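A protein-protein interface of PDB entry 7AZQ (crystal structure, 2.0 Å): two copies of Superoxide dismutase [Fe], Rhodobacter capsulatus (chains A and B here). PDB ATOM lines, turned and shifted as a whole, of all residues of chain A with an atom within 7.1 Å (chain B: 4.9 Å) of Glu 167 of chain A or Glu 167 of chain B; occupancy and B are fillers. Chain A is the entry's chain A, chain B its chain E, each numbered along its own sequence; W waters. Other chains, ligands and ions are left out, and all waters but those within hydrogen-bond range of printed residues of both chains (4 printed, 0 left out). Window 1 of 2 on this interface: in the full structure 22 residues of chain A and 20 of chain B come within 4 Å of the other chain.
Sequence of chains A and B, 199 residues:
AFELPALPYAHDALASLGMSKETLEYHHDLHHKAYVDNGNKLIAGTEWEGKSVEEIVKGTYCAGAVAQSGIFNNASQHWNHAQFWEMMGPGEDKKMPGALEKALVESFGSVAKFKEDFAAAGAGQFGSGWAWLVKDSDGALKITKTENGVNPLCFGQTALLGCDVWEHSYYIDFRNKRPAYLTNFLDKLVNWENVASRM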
ATOM      1  N   HIS A  31      -4.390 -18.778  33.018  1.00  0.00           N
ATOM      2  CA  HIS A  31      -5.669 -18.056  32.902  1.00  0.00           C
ATOM      3  C   HIS A  31      -6.848 -19.035  33.146  1.00  0.00           C
ATOM      4  O   HIS A  31      -7.732 -18.776  33.944  1.00  0.00           O
ATOM      5  CB  HIS A  31      -5.836 -17.357  31.550  1.00  0.00           C
ATOM      6  CG  HIS A  31      -4.958 -16.162  31.352  1.00  0.00           C
ATOM      7  ND1 HIS A  31      -5.375 -14.872  31.619  1.00  0.00           N
ATOM      8  CD2 HIS A  31      -3.721 -16.052  30.819  1.00  0.00           C
ATOM      9  CE1 HIS A  31      -4.404 -14.030  31.315  1.00  0.00           C
ATOM     10  NE2 HIS A  31      -3.392 -14.719  30.815  1.00  0.00           N
ATOM     11  N   TYR A  35      -9.784 -19.303  36.341  1.00  0.00           N
ATOM     12  CA  TYR A  35     -11.246 -19.405  36.270  1.00  0.00           C
ATOM     13  C   TYR A  35     -11.758 -20.598  37.051  1.00  0.00           C
ATOM     14  O   TYR A  35     -12.772 -20.505  37.730  1.00  0.00           O
ATOM     15  CB  TYR A  35     -11.772 -19.482  34.825  1.00  0.00           C
ATOM     16  CG  TYR A  35     -11.273 -18.360  33.943  1.00  0.00           C
ATOM     17  CD1 TYR A  35     -11.393 -17.033  34.336  1.00  0.00           C
ATOM     18  CD2 TYR A  35     -10.671 -18.638  32.710  1.00  0.00           C
ATOM     19  CE1 TYR A  35     -10.943 -15.995  33.529  1.00  0.00           C
ATOM     20  CE2 TYR A  35     -10.196 -17.614  31.902  1.00  0.00           C
ATOM     21  CZ  TYR A  35     -10.337 -16.302  32.304  1.00  0.00           C
ATOM     22  OH  TYR A  35      -9.889 -15.272  31.548  1.00  0.00           O
ATOM     23  N   GLY A 127     -12.913  -4.306  23.479  1.00  0.00           N
ATOM     24  CA  GLY A 127     -12.415  -4.749  24.767  1.00  0.00           C
ATOM     25  C   GLY A 127     -12.239  -6.285  24.720  1.00  0.00           C
ATOM     26  O   GLY A 127     -11.773  -6.833  23.702  1.00  0.00           O
ATOM     27  N   SER A 128     -12.619  -6.959  25.809  1.00  0.00           N
ATOM     28  CA  SER A 128     -12.418  -8.407  25.968  1.00  0.00           C
ATOM     29  C   SER A 128     -13.679  -9.123  25.548  1.00  0.00           C
ATOM     30  O   SER A 128     -14.799  -8.621  25.784  1.00  0.00           O
ATOM     31  CB  SER A 128     -12.094  -8.778  27.415  1.00  0.00           C
ATOM     32  OG  SER A 128     -10.921  -8.158  27.869  1.00  0.00           O
ATOM     33  N   GLY A 129     -13.516 -10.305  24.948  1.00  0.00           N
ATOM     34  CA  GLY A 129     -14.662 -11.162  24.651  1.00  0.00           C
ATOM     35  C   GLY A 129     -14.379 -12.264  23.685  1.00  0.00           C
ATOM     36  O   GLY A 129     -13.236 -12.774  23.643  1.00  0.00           O
ATOM     37  N   ASP A 164     -11.515 -16.764  21.262  1.00  0.00           N
ATOM     38  CA  ASP A 164     -11.196 -15.866  22.361  1.00  0.00           C
ATOM     39  C   ASP A 164     -10.534 -14.635  21.766  1.00  0.00           C
ATOM     40  O   ASP A 164      -9.505 -14.748  21.092  1.00  0.00           O
ATOM     41  CB  ASP A 164     -10.243 -16.595  23.261  1.00  0.00           C
ATOM     42  CG  ASP A 164     -10.028 -15.922  24.593  1.00  0.00           C
ATOM     43  OD1 ASP A 164     -10.543 -14.827  24.803  1.00  0.00           O
ATOM     44  OD2 ASP A 164      -9.282 -16.510  25.375  1.00  0.00           O
ATOM     45  N   VAL A 165     -11.161 -13.470  21.919  1.00  0.00           N
ATOM     46  CA  VAL A 165     -10.484 -12.235  21.536  1.00  0.00           C
ATOM     47  C   VAL A 165     -10.058 -11.360  22.744  1.00  0.00           C
ATOM     48  O   VAL A 165      -9.756 -10.179  22.583  1.00  0.00           O
ATOM     49  CB  VAL A 165     -11.292 -11.433  20.502  1.00  0.00           C
ATOM     50  CG1 VAL A 165     -11.429 -12.238  19.196  1.00  0.00           C
ATOM     51  CG2 VAL A 165     -12.638 -11.035  21.025  1.00  0.00           C
ATOM     52  N   TRP A 166     -10.034 -11.940  23.953  1.00  0.00           N
ATOM     53  CA  TRP A 166      -9.289 -11.294  25.036  1.00  0.00           C
ATOM     54  C   TRP A 166      -7.837 -11.210  24.532  1.00  0.00           C
ATOM     55  O   TRP A 166      -7.344 -12.141  23.879  1.00  0.00           O
ATOM     56  CB  TRP A 166      -9.302 -12.123  26.306  1.00  0.00           C
ATOM     57  CG  TRP A 166     -10.560 -12.146  27.093  1.00  0.00           C
ATOM     58  CD1 TRP A 166     -11.767 -12.543  26.677  1.00  0.00           C
ATOM     59  CD2 TRP A 166     -10.685 -11.855  28.503  1.00  0.00           C
ATOM     60  NE1 TRP A 166     -12.669 -12.490  27.713  1.00  0.00           N
ATOM     61  CE2 TRP A 166     -12.035 -12.044  28.843  1.00  0.00           C
ATOM     62  CE3 TRP A 166      -9.801 -11.392  29.480  1.00  0.00           C
ATOM     63  CZ2 TRP A 166     -12.519 -11.823  30.105  1.00  0.00           C
ATOM     64  CZ3 TRP A 166     -10.284 -11.160  30.755  1.00  0.00           C
ATOM     65  CH2 TRP A 166     -11.621 -11.408  31.062  1.00  0.00           C
ATOM     66  N   GLU A 167      -7.152 -10.119  24.859  1.00  0.00           N
ATOM     67  CA  GLU A 167      -5.813  -9.873  24.347  1.00  0.00           C
ATOM     68  C   GLU A 167      -4.790 -10.963  24.744  1.00  0.00           C
ATOM     69  O   GLU A 167      -3.907 -11.306  23.944  1.00  0.00           O
ATOM     70  CB  GLU A 167      -5.349  -8.466  24.740  1.00  0.00           C
ATOM     71  CG  GLU A 167      -6.054  -7.404  23.896  1.00  0.00           C
ATOM     72  CD  GLU A 167      -5.771  -5.984  24.310  1.00  0.00           C
ATOM     73  OE1 GLU A 167      -5.662  -5.727  25.531  1.00  0.00           O
ATOM     74  OE2 GLU A 167      -5.610  -5.148  23.397  1.00  0.00           O
ATOM     75  N   HIS A 168      -4.954 -11.557  25.932  1.00  0.00           N
ATOM     76  CA  HIS A 168      -4.087 -12.656  26.375  1.00  0.00           C
ATOM     77  C   HIS A 168      -4.064 -13.820  25.359  1.00  0.00           C
ATOM     78  O   HIS A 168      -3.093 -14.533  25.272  1.00  0.00           O
ATOM     79  CB  HIS A 168      -4.437 -13.180  27.772  1.00  0.00           C
ATOM     80  CG  HIS A 168      -5.803 -13.828  27.905  1.00  0.00           C
ATOM     81  ND1 HIS A 168      -6.748 -13.377  28.800  1.00  0.00           N
ATOM     82  CD2 HIS A 168      -6.337 -14.951  27.336  1.00  0.00           C
ATOM     83  CE1 HIS A 168      -7.828 -14.149  28.723  1.00  0.00           C
ATOM     84  NE2 HIS A 168      -7.606 -15.134  27.857  1.00  0.00           N
ATOM     85  N   SER A 169      -5.161 -14.004  24.623  1.00  0.00           N
ATOM     86  CA  SER A 169      -5.259 -15.111  23.695  1.00  0.00           C
ATOM     87  C   SER A 169      -4.312 -14.993  22.508  1.00  0.00           C
ATOM     88  O   SER A 169      -3.960 -16.011  21.914  1.00  0.00           O
ATOM     89  CB  SER A 169      -6.691 -15.289  23.174  1.00  0.00           C
ATOM     90  OG  SER A 169      -6.796 -16.597  22.641  1.00  0.00           O
ATOM     91  N   TYR A 170      -3.911 -13.763  22.162  1.00  0.00           N
ATOM     92  CA  TYR A 170      -3.103 -13.521  20.989  1.00  0.00           C
ATOM     93  C   TYR A 170      -1.922 -12.601  21.125  1.00  0.00           C
ATOM     94  O   TYR A 170      -1.088 -12.581  20.240  1.00  0.00           O
ATOM     95  CB  TYR A 170      -3.989 -13.004  19.854  1.00  0.00           C
ATOM     96  CG  TYR A 170      -4.728 -11.692  20.106  1.00  0.00           C
ATOM     97  CD1 TYR A 170      -4.141 -10.467  19.808  1.00  0.00           C
ATOM     98  CD2 TYR A 170      -6.016 -11.681  20.618  1.00  0.00           C
ATOM     99  CE1 TYR A 170      -4.818  -9.281  19.985  1.00  0.00           C
ATOM    100  CE2 TYR A 170      -6.703 -10.491  20.812  1.00  0.00           C
ATOM    101  CZ  TYR A 170      -6.098  -9.299  20.480  1.00  0.00           C
ATOM    102  OH  TYR A 170      -6.774  -8.119  20.690  1.00  0.00           O
ATOM    103  N   TYR A 171      -1.834 -11.847  22.229  1.00  0.00           N
ATOM    104  CA  TYR A 171      -0.868 -10.763  22.336  1.00  0.00           C
ATOM    105  C   TYR A 171       0.580 -11.257  22.253  1.00  0.00           C
ATOM    106  O   TYR A 171       1.444 -10.555  21.720  1.00  0.00           O
ATOM    107  CB  TYR A 171      -1.089  -9.907  23.597  1.00  0.00           C
ATOM    108  CG  TYR A 171      -0.848  -8.445  23.318  1.00  0.00           C
ATOM    109  CD1 TYR A 171      -1.784  -7.688  22.592  1.00  0.00           C
ATOM    110  CD2 TYR A 171       0.333  -7.830  23.694  1.00  0.00           C
ATOM    111  CE1 TYR A 171      -1.549  -6.359  22.288  1.00  0.00           C
ATOM    112  CE2 TYR A 171       0.573  -6.489  23.410  1.00  0.00           C
ATOM    113  CZ  TYR A 171      -0.378  -5.756  22.706  1.00  0.00           C
ATOM    114  OH  TYR A 171      -0.119  -4.447  22.388  1.00  0.00           O
ATOM    115  N   ILE A 172       0.844 -12.471  22.753  1.00  0.00           N
ATOM    116  CA  ILE A 172       2.201 -13.022  22.715  1.00  0.00           C
ATOM    117  C   ILE A 172       2.621 -13.254  21.272  1.00  0.00           C
ATOM    118  O   ILE A 172       3.741 -12.955  20.918  1.00  0.00           O
ATOM    119  CB  ILE A 172       2.355 -14.332  23.526  1.00  0.00           C
ATOM    120  CG1 ILE A 172       2.175 -14.049  25.035  1.00  0.00           C
ATOM    121  CG2 ILE A 172       3.739 -14.959  23.279  1.00  0.00           C
ATOM    122  CD1 ILE A 172       1.747 -15.265  25.832  1.00  0.00           C
ATOM    123  N   ASP A 173       1.696 -13.754  20.445  1.00  0.00           N
ATOM    124  CA  ASP A 173       2.017 -14.203  19.102  1.00  0.00           C
ATOM    125  C   ASP A 173       1.761 -13.147  18.017  1.00  0.00           C
ATOM    126  O   ASP A 173       2.451 -13.144  17.018  1.00  0.00           O
ATOM    127  CB  ASP A 173       1.229 -15.472  18.793  1.00  0.00           C
ATOM    128  CG  ASP A 173       1.516 -16.582  19.780  1.00  0.00           C
ATOM    129  OD1 ASP A 173       2.672 -16.686  20.230  1.00  0.00           O
ATOM    130  OD2 ASP A 173       0.569 -17.309  20.154  1.00  0.00           O
ATOM    131  N   ARG A 175       0.707  -9.608  19.011  1.00  0.00           N
ATOM    132  CA  ARG A 175       0.565  -8.287  19.643  1.00  0.00           C
ATOM    133  C   ARG A 175      -0.841  -7.709  19.341  1.00  0.00           C
ATOM    134  O   ARG A 175      -1.834  -8.378  19.569  1.00  0.00           O
ATOM    135  CB  ARG A 175       1.719  -7.377  19.191  1.00  0.00           C
ATOM    136  CG  ARG A 175       3.084  -7.852  19.676  1.00  0.00           C
ATOM    137  CD  ARG A 175       3.293  -7.516  21.157  1.00  0.00           C
ATOM    138  NE  ARG A 175       4.650  -7.848  21.575  1.00  0.00           N
ATOM    139  CZ  ARG A 175       5.060  -9.055  21.950  1.00  0.00           C
ATOM    140  NH1 ARG A 175       4.216 -10.091  21.990  1.00  0.00           N
ATOM    141  NH2 ARG A 175       6.351  -9.232  22.260  1.00  0.00           N
ATOM    142  N   ASN A 176      -0.901  -6.488  18.803  1.00  0.00           N
ATOM    143  CA  ASN A 176      -2.158  -5.771  18.547  1.00  0.00           C
ATOM    144  C   ASN A 176      -2.948  -6.259  17.344  1.00  0.00           C
ATOM    145  O   ASN A 176      -4.065  -5.797  17.109  1.00  0.00           O
ATOM    146  CB  ASN A 176      -1.840  -4.281  18.304  1.00  0.00           C
ATOM    147  CG  ASN A 176      -0.996  -4.079  17.096  1.00  0.00           C
ATOM    148  OD1 ASN A 176       0.123  -4.529  17.055  1.00  0.00           O
ATOM    149  ND2 ASN A 176      -1.539  -3.451  16.088  1.00  0.00           N
ATOM    150  N   ARG A 178      -5.134  -8.273  16.099  1.00  0.00           N
ATOM    151  CA  ARG A 178      -6.254  -9.155  16.321  1.00  0.00           C
ATOM    152  C   ARG A 178      -6.819  -9.685  15.003  1.00  0.00           C
ATOM    153  O   ARG A 178      -7.141 -10.868  14.930  1.00  0.00           O
ATOM    154  CB  ARG A 178      -7.332  -8.472  17.152  1.00  0.00           C
ATOM    155  CG  ARG A 178      -8.391  -9.454  17.619  1.00  0.00           C
ATOM    156  CD  ARG A 178      -9.633  -8.746  18.140  1.00  0.00           C
ATOM    157  NE  ARG A 178      -9.405  -8.230  19.475  1.00  0.00           N
ATOM    158  CZ  ARG A 178     -10.360  -7.661  20.191  1.00  0.00           C
ATOM    159  NH1 ARG A 178     -11.613  -7.613  19.741  1.00  0.00           N
ATOM    160  NH2 ARG A 178     -10.088  -7.230  21.391  1.00  0.00           N
ATOM    161  N   HIS B  31      -1.868   1.274  19.384  1.00  0.00           N
ATOM    162  CA  HIS B  31      -3.199   1.256  20.007  1.00  0.00           C
ATOM    163  C   HIS B  31      -3.801   2.662  20.077  1.00  0.00           C
ATOM    164  O   HIS B  31      -4.921   2.886  19.663  1.00  0.00           O
ATOM    165  CB  HIS B  31      -3.181   0.632  21.424  1.00  0.00           C
ATOM    166  CG  HIS B  31      -2.956  -0.845  21.448  1.00  0.00           C
ATOM    167  ND1 HIS B  31      -3.998  -1.746  21.458  1.00  0.00           N
ATOM    168  CD2 HIS B  31      -1.813  -1.583  21.465  1.00  0.00           C
ATOM    169  CE1 HIS B  31      -3.511  -2.976  21.488  1.00  0.00           C
ATOM    170  NE2 HIS B  31      -2.185  -2.909  21.483  1.00  0.00           N
ATOM    171  N   VAL B 165      -6.060  -1.088  32.564  1.00  0.00           N
ATOM    172  CA  VAL B 165      -5.970  -2.520  32.833  1.00  0.00           C
ATOM    173  C   VAL B 165      -6.426  -3.394  31.649  1.00  0.00           C
ATOM    174  O   VAL B 165      -6.616  -4.596  31.800  1.00  0.00           O
ATOM    175  CB  VAL B 165      -6.624  -2.938  34.151  1.00  0.00           C
ATOM    176  CG1 VAL B 165      -5.914  -2.265  35.323  1.00  0.00           C
ATOM    177  CG2 VAL B 165      -8.111  -2.607  34.157  1.00  0.00           C
ATOM    178  N   TRP B 166      -6.566  -2.803  30.472  1.00  0.00           N
ATOM    179  CA  TRP B 166      -6.549  -3.643  29.262  1.00  0.00           C
ATOM    180  C   TRP B 166      -5.241  -4.426  29.273  1.00  0.00           C
ATOM    181  O   TRP B 166      -4.191  -3.888  29.619  1.00  0.00           O
ATOM    182  CB  TRP B 166      -6.609  -2.842  27.987  1.00  0.00           C
ATOM    183  CG  TRP B 166      -7.911  -2.153  27.668  1.00  0.00           C
ATOM    184  CD1 TRP B 166      -8.572  -1.234  28.435  1.00  0.00           C
ATOM    185  CD2 TRP B 166      -8.630  -2.242  26.432  1.00  0.00           C
ATOM    186  NE1 TRP B 166      -9.664  -0.762  27.766  1.00  0.00           N
ATOM    187  CE2 TRP B 166      -9.730  -1.355  26.531  1.00  0.00           C
ATOM    188  CE3 TRP B 166      -8.449  -2.970  25.260  1.00  0.00           C
ATOM    189  CZ2 TRP B 166     -10.654  -1.192  25.511  1.00  0.00           C
ATOM    190  CZ3 TRP B 166      -9.385  -2.792  24.213  1.00  0.00           C
ATOM    191  CH2 TRP B 166     -10.461  -1.915  24.353  1.00  0.00           C
ATOM    192  N   GLU B 167      -5.308  -5.707  28.885  1.00  0.00           N
ATOM    193  CA  GLU B 167      -4.141  -6.576  28.894  1.00  0.00           C
ATOM    194  C   GLU B 167      -2.965  -6.058  28.052  1.00  0.00           C
ATOM    195  O   GLU B 167      -1.803  -6.243  28.448  1.00  0.00           O
ATOM    196  CB  GLU B 167      -4.543  -8.001  28.522  1.00  0.00           C
ATOM    197  CG  GLU B 167      -5.393  -8.669  29.594  1.00  0.00           C
ATOM    198  CD  GLU B 167      -5.888 -10.031  29.189  1.00  0.00           C
ATOM    199  OE1 GLU B 167      -6.393 -10.145  28.037  1.00  0.00           O
ATOM    200  OE2 GLU B 167      -5.763 -10.986  30.008  1.00  0.00           O
ATOM    201  N   HIS B 168      -3.254  -5.323  26.966  1.00  0.00           N
ATOM    202  CA  HIS B 168      -2.143  -4.759  26.134  1.00  0.00           C
ATOM    203  C   HIS B 168      -1.247  -3.842  26.959  1.00  0.00           C
ATOM    204  O   HIS B 168      -0.069  -3.670  26.647  1.00  0.00           O
ATOM    205  CB  HIS B 168      -2.613  -4.006  24.864  1.00  0.00           C
ATOM    206  CG  HIS B 168      -3.475  -2.795  25.124  1.00  0.00           C
ATOM    207  ND1 HIS B 168      -4.785  -2.723  24.693  1.00  0.00           N
ATOM    208  CD2 HIS B 168      -3.210  -1.617  25.754  1.00  0.00           C
ATOM    209  CE1 HIS B 168      -5.293  -1.561  25.078  1.00  0.00           C
ATOM    210  NE2 HIS B 168      -4.363  -0.861  25.738  1.00  0.00           N
ATOM    211  N   SER B 169      -1.816  -3.207  27.991  1.00  0.00           N
ATOM    212  CA  SER B 169      -1.050  -2.265  28.803  1.00  0.00           C
ATOM    213  C   SER B 169       0.080  -2.919  29.595  1.00  0.00           C
ATOM    214  O   SER B 169       1.041  -2.246  29.933  1.00  0.00           O
ATOM    215  CB  SER B 169      -1.954  -1.478  29.758  1.00  0.00           C
ATOM    216  OG  SER B 169      -1.263  -0.315  30.183  1.00  0.00           O
ATOM    217  N   TYR B 170      -0.061  -4.220  29.902  1.00  0.00           N
ATOM    218  CA  TYR B 170       0.883  -4.916  30.752  1.00  0.00           C
ATOM    219  C   TYR B 170       1.365  -6.274  30.318  1.00  0.00           C
ATOM    220  O   TYR B 170       2.337  -6.767  30.866  1.00  0.00           O
ATOM    221  CB  TYR B 170       0.307  -5.037  32.171  1.00  0.00           C
ATOM    222  CG  TYR B 170      -0.995  -5.837  32.300  1.00  0.00           C
ATOM    223  CD1 TYR B 170      -0.983  -7.213  32.507  1.00  0.00           C
ATOM    224  CD2 TYR B 170      -2.217  -5.206  32.255  1.00  0.00           C
ATOM    225  CE1 TYR B 170      -2.160  -7.932  32.676  1.00  0.00           C
ATOM    226  CE2 TYR B 170      -3.397  -5.918  32.425  1.00  0.00           C
ATOM    227  CZ  TYR B 170      -3.356  -7.278  32.632  1.00  0.00           C
ATOM    228  OH  TYR B 170      -4.541  -7.958  32.797  1.00  0.00           O
ATOM    229  N   TYR B 171       0.712  -6.882  29.324  1.00  0.00           N
ATOM    230  CA  TYR B 171       0.989  -8.283  28.986  1.00  0.00           C
ATOM    231  C   TYR B 171       2.433  -8.532  28.527  1.00  0.00           C
ATOM    232  O   TYR B 171       3.012  -9.593  28.801  1.00  0.00           O
ATOM    233  CB  TYR B 171      -0.029  -8.833  27.986  1.00  0.00           C
ATOM    234  CG  TYR B 171      -0.365 -10.270  28.273  1.00  0.00           C
ATOM    235  CD1 TYR B 171      -1.237 -10.586  29.312  1.00  0.00           C
ATOM    236  CD2 TYR B 171       0.212 -11.321  27.545  1.00  0.00           C
ATOM    237  CE1 TYR B 171      -1.528 -11.906  29.629  1.00  0.00           C
ATOM    238  CE2 TYR B 171      -0.102 -12.636  27.835  1.00  0.00           C
ATOM    239  CZ  TYR B 171      -0.971 -12.928  28.890  1.00  0.00           C
ATOM    240  OH  TYR B 171      -1.304 -14.234  29.193  1.00  0.00           O
ATOM    241  N   ARG B 178      -1.495  -9.001  36.498  1.00  0.00           N
ATOM    242  CA  ARG B 178      -2.099  -7.697  36.623  1.00  0.00           C
ATOM    243  C   ARG B 178      -1.870  -7.077  38.012  1.00  0.00           C
ATOM    244  O   ARG B 178      -1.573  -5.889  38.096  1.00  0.00           O
ATOM    245  CB  ARG B 178      -3.600  -7.730  36.278  1.00  0.00           C
ATOM    246  CG  ARG B 178      -4.150  -6.319  36.121  1.00  0.00           C
ATOM    247  CD  ARG B 178      -5.657  -6.263  36.087  1.00  0.00           C
ATOM    248  NE  ARG B 178      -6.190  -6.738  34.823  1.00  0.00           N
ATOM    249  CZ  ARG B 178      -7.478  -6.704  34.513  1.00  0.00           C
ATOM    250  NH1 ARG B 178      -8.348  -6.202  35.375  1.00  0.00           N
ATOM    251  NH2 ARG B 178      -7.879  -7.145  33.345  1.00  0.00           N
HETATM  252  O   HOH W   1      -7.724  -6.180  27.263  1.00  0.00           O
HETATM  253  O   HOH W   2      -8.377  -8.686  27.162  1.00  0.00           O
HETATM  254  O   HOH W   3       0.981  -2.632  24.283  1.00  0.00           O
HETATM  255  O   HOH W   4      -1.942 -16.159  27.333  1.00  0.00           O
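A ring nitrogen (ND1) of His 168 of chain A is in hydrogen-bond range of the side-chain carboxylate (OE2) of Glu 167 of chain B, 2.9 Å away.
NE2 of His 31 of chain A is in hydrogen-bond range of OH of Tyr 171 of chain B, at 2.7 Å.
OE1 of Glu 167 of chain B sits at hydrogen-bond distance from N of Glu 167 of chain A (3.3 Å).
OE1 of Glu 167 of chain A is in hydrogen-bond range of N of His 168 of chain B, at 2.8 Å.
OH of Tyr 171 of chain A is in hydrogen-bond range of NE2 of His 31 of chain B.
ND1 of His 168 of chain A lies within hydrogen-bond range of ND1 of His 31 of chain A (3.5 Å).
The backbone carbonyl oxygen (O) of Tyr 171 of chain A sits at hydrogen-bond distance from the guanidinium group (NH1) of Arg 175 of chain A (2.8 Å).
A ring nitrogen (ND1) of His 168 of chain B sits close to a ring nitrogen (ND1) of His 31 of chain B, 3.5 Å away.
OD1 of Asp 164 of chain A sits at hydrogen-bond distance from N of Trp 166 of chain A, at 3.1 Å.
The backbone carbonyl oxygen of Gly 129 of chain A sits at hydrogen-bond distance from the backbone NH of Trp 166 of chain A, 3.3 Å away.
The backbone carbonyl oxygen of Ile 172 of chain A sits at hydrogen-bond distance from the guanidinium group of Arg 175 of chain A (3.1 Å).
CE1 of His 31 of chain A touches OE2 of Glu 167 of chain B (3.6 Å).
CA of Gly 127 of chain A touches CH2 of Trp 166 of chain B, 3.5 Å away.
Trp 166 of chain A touches Glu 167 of chain B.
OE2 of Glu 167 of chain A touches CE1 of His 31 of chain B (3.6 Å).
Glu 167 of chain A touches Trp 166 of chain B (OE1 to CB, 3.9 Å).
His 168 of chain A touches Tyr 171 of chain B.
His 168 of chain B touches Tyr 171 of chain A.
Ile 172 of chain A touches Tyr 171 of chain B.
His 31 of chain B touches Asn 176 of chain A (NE2 to CB, 3.5 Å).
Printed residues of chain B within 4 Å of Gly 127 of chain A: Trp 166.
Gly 129 of chain A touches none of the printed residues of chain B.
Printed residues of chain B within 4 Å of Trp 166 of chain A: Glu 167 (3.9 Å).
Glu 167 of chain A touches four residues of chain B.
Arg 178 of chain A touches none of the printed residues of chain B.
Printed residues of chain A within 4 Å of Trp 166 of chain B: Gly 127 and Glu 167.
Glu 167 of chain B touches just these residues of chain A: His 31 (3.6 Å), Trp 166 (3.9 Å), Glu 167 (3.3 Å) and His 168 (2.9 Å).
Of the printed residues of chain A, Tyr 171 of chain B touches His 31, His 168 and Ile 172.
The nearest printed residue of chain B that does not touch Glu 167 of chain A is Ser 169 of chain B (5.2 Å).
Hydrophobic or aromatic side chains of chain A within 4 Å of the printed part of chain B: His 31, Trp 166, His 168, Tyr 171 and Ile 172.
Of the 9 printed residues of chain B, 5 touch a printed residue of chain A.
Printed residues of chain B that touch a printed residue of chain A: His 31, Trp 166, Glu 167, His 168 and Tyr 171.
Among the printed residues, no Asp or Glu carboxylate lies within 4 Å of a Lys or Arg side-chain nitrogen of the other chain.
His 31 of chain A touches Glu 167 of chain B, and with the chains exchanged Glu 167 of chain A touches His 31 of chain B.
His 31 of chain A touches Tyr 171 of chain B, and with the chains exchanged Tyr 171 of chain A touches His 31 of chain B.
Glu 167 of chain A touches its own counterpart, Glu 167 of chain B.
Glu 167 of chain A touches His 168 of chain B, and with the chains exchanged His 168 of chain A touches Glu 167 of chain B.
9 positions are printed for both chains.
Of the 14 pairs that touch across the chains among the printed residues, 11 have their exchanged pair printed and touching as well.
Water W2 lies within hydrogen-bond range of the side-chain carboxylate of Glu 167 of chain B (2.6 Å), the side-chain hydroxyl of Ser 128 of chain A (2.7 Å) and the backbone NH of Glu 167 of chain A (3.0 Å).
Water W1 lies within hydrogen-bond range of the side-chain carboxylate of Glu 167 of chain A (2.7 Å) and the backbone NH of Glu 167 of chain B (2.9 Å).
Water W4 bridges OH of Tyr 171 of chain B and O of His 168 of chain A.
Water W3 lies within hydrogen-bond range of O of His 168 of chain B (2.8 Å) and OH of Tyr 171 of chain A (2.8 Å).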
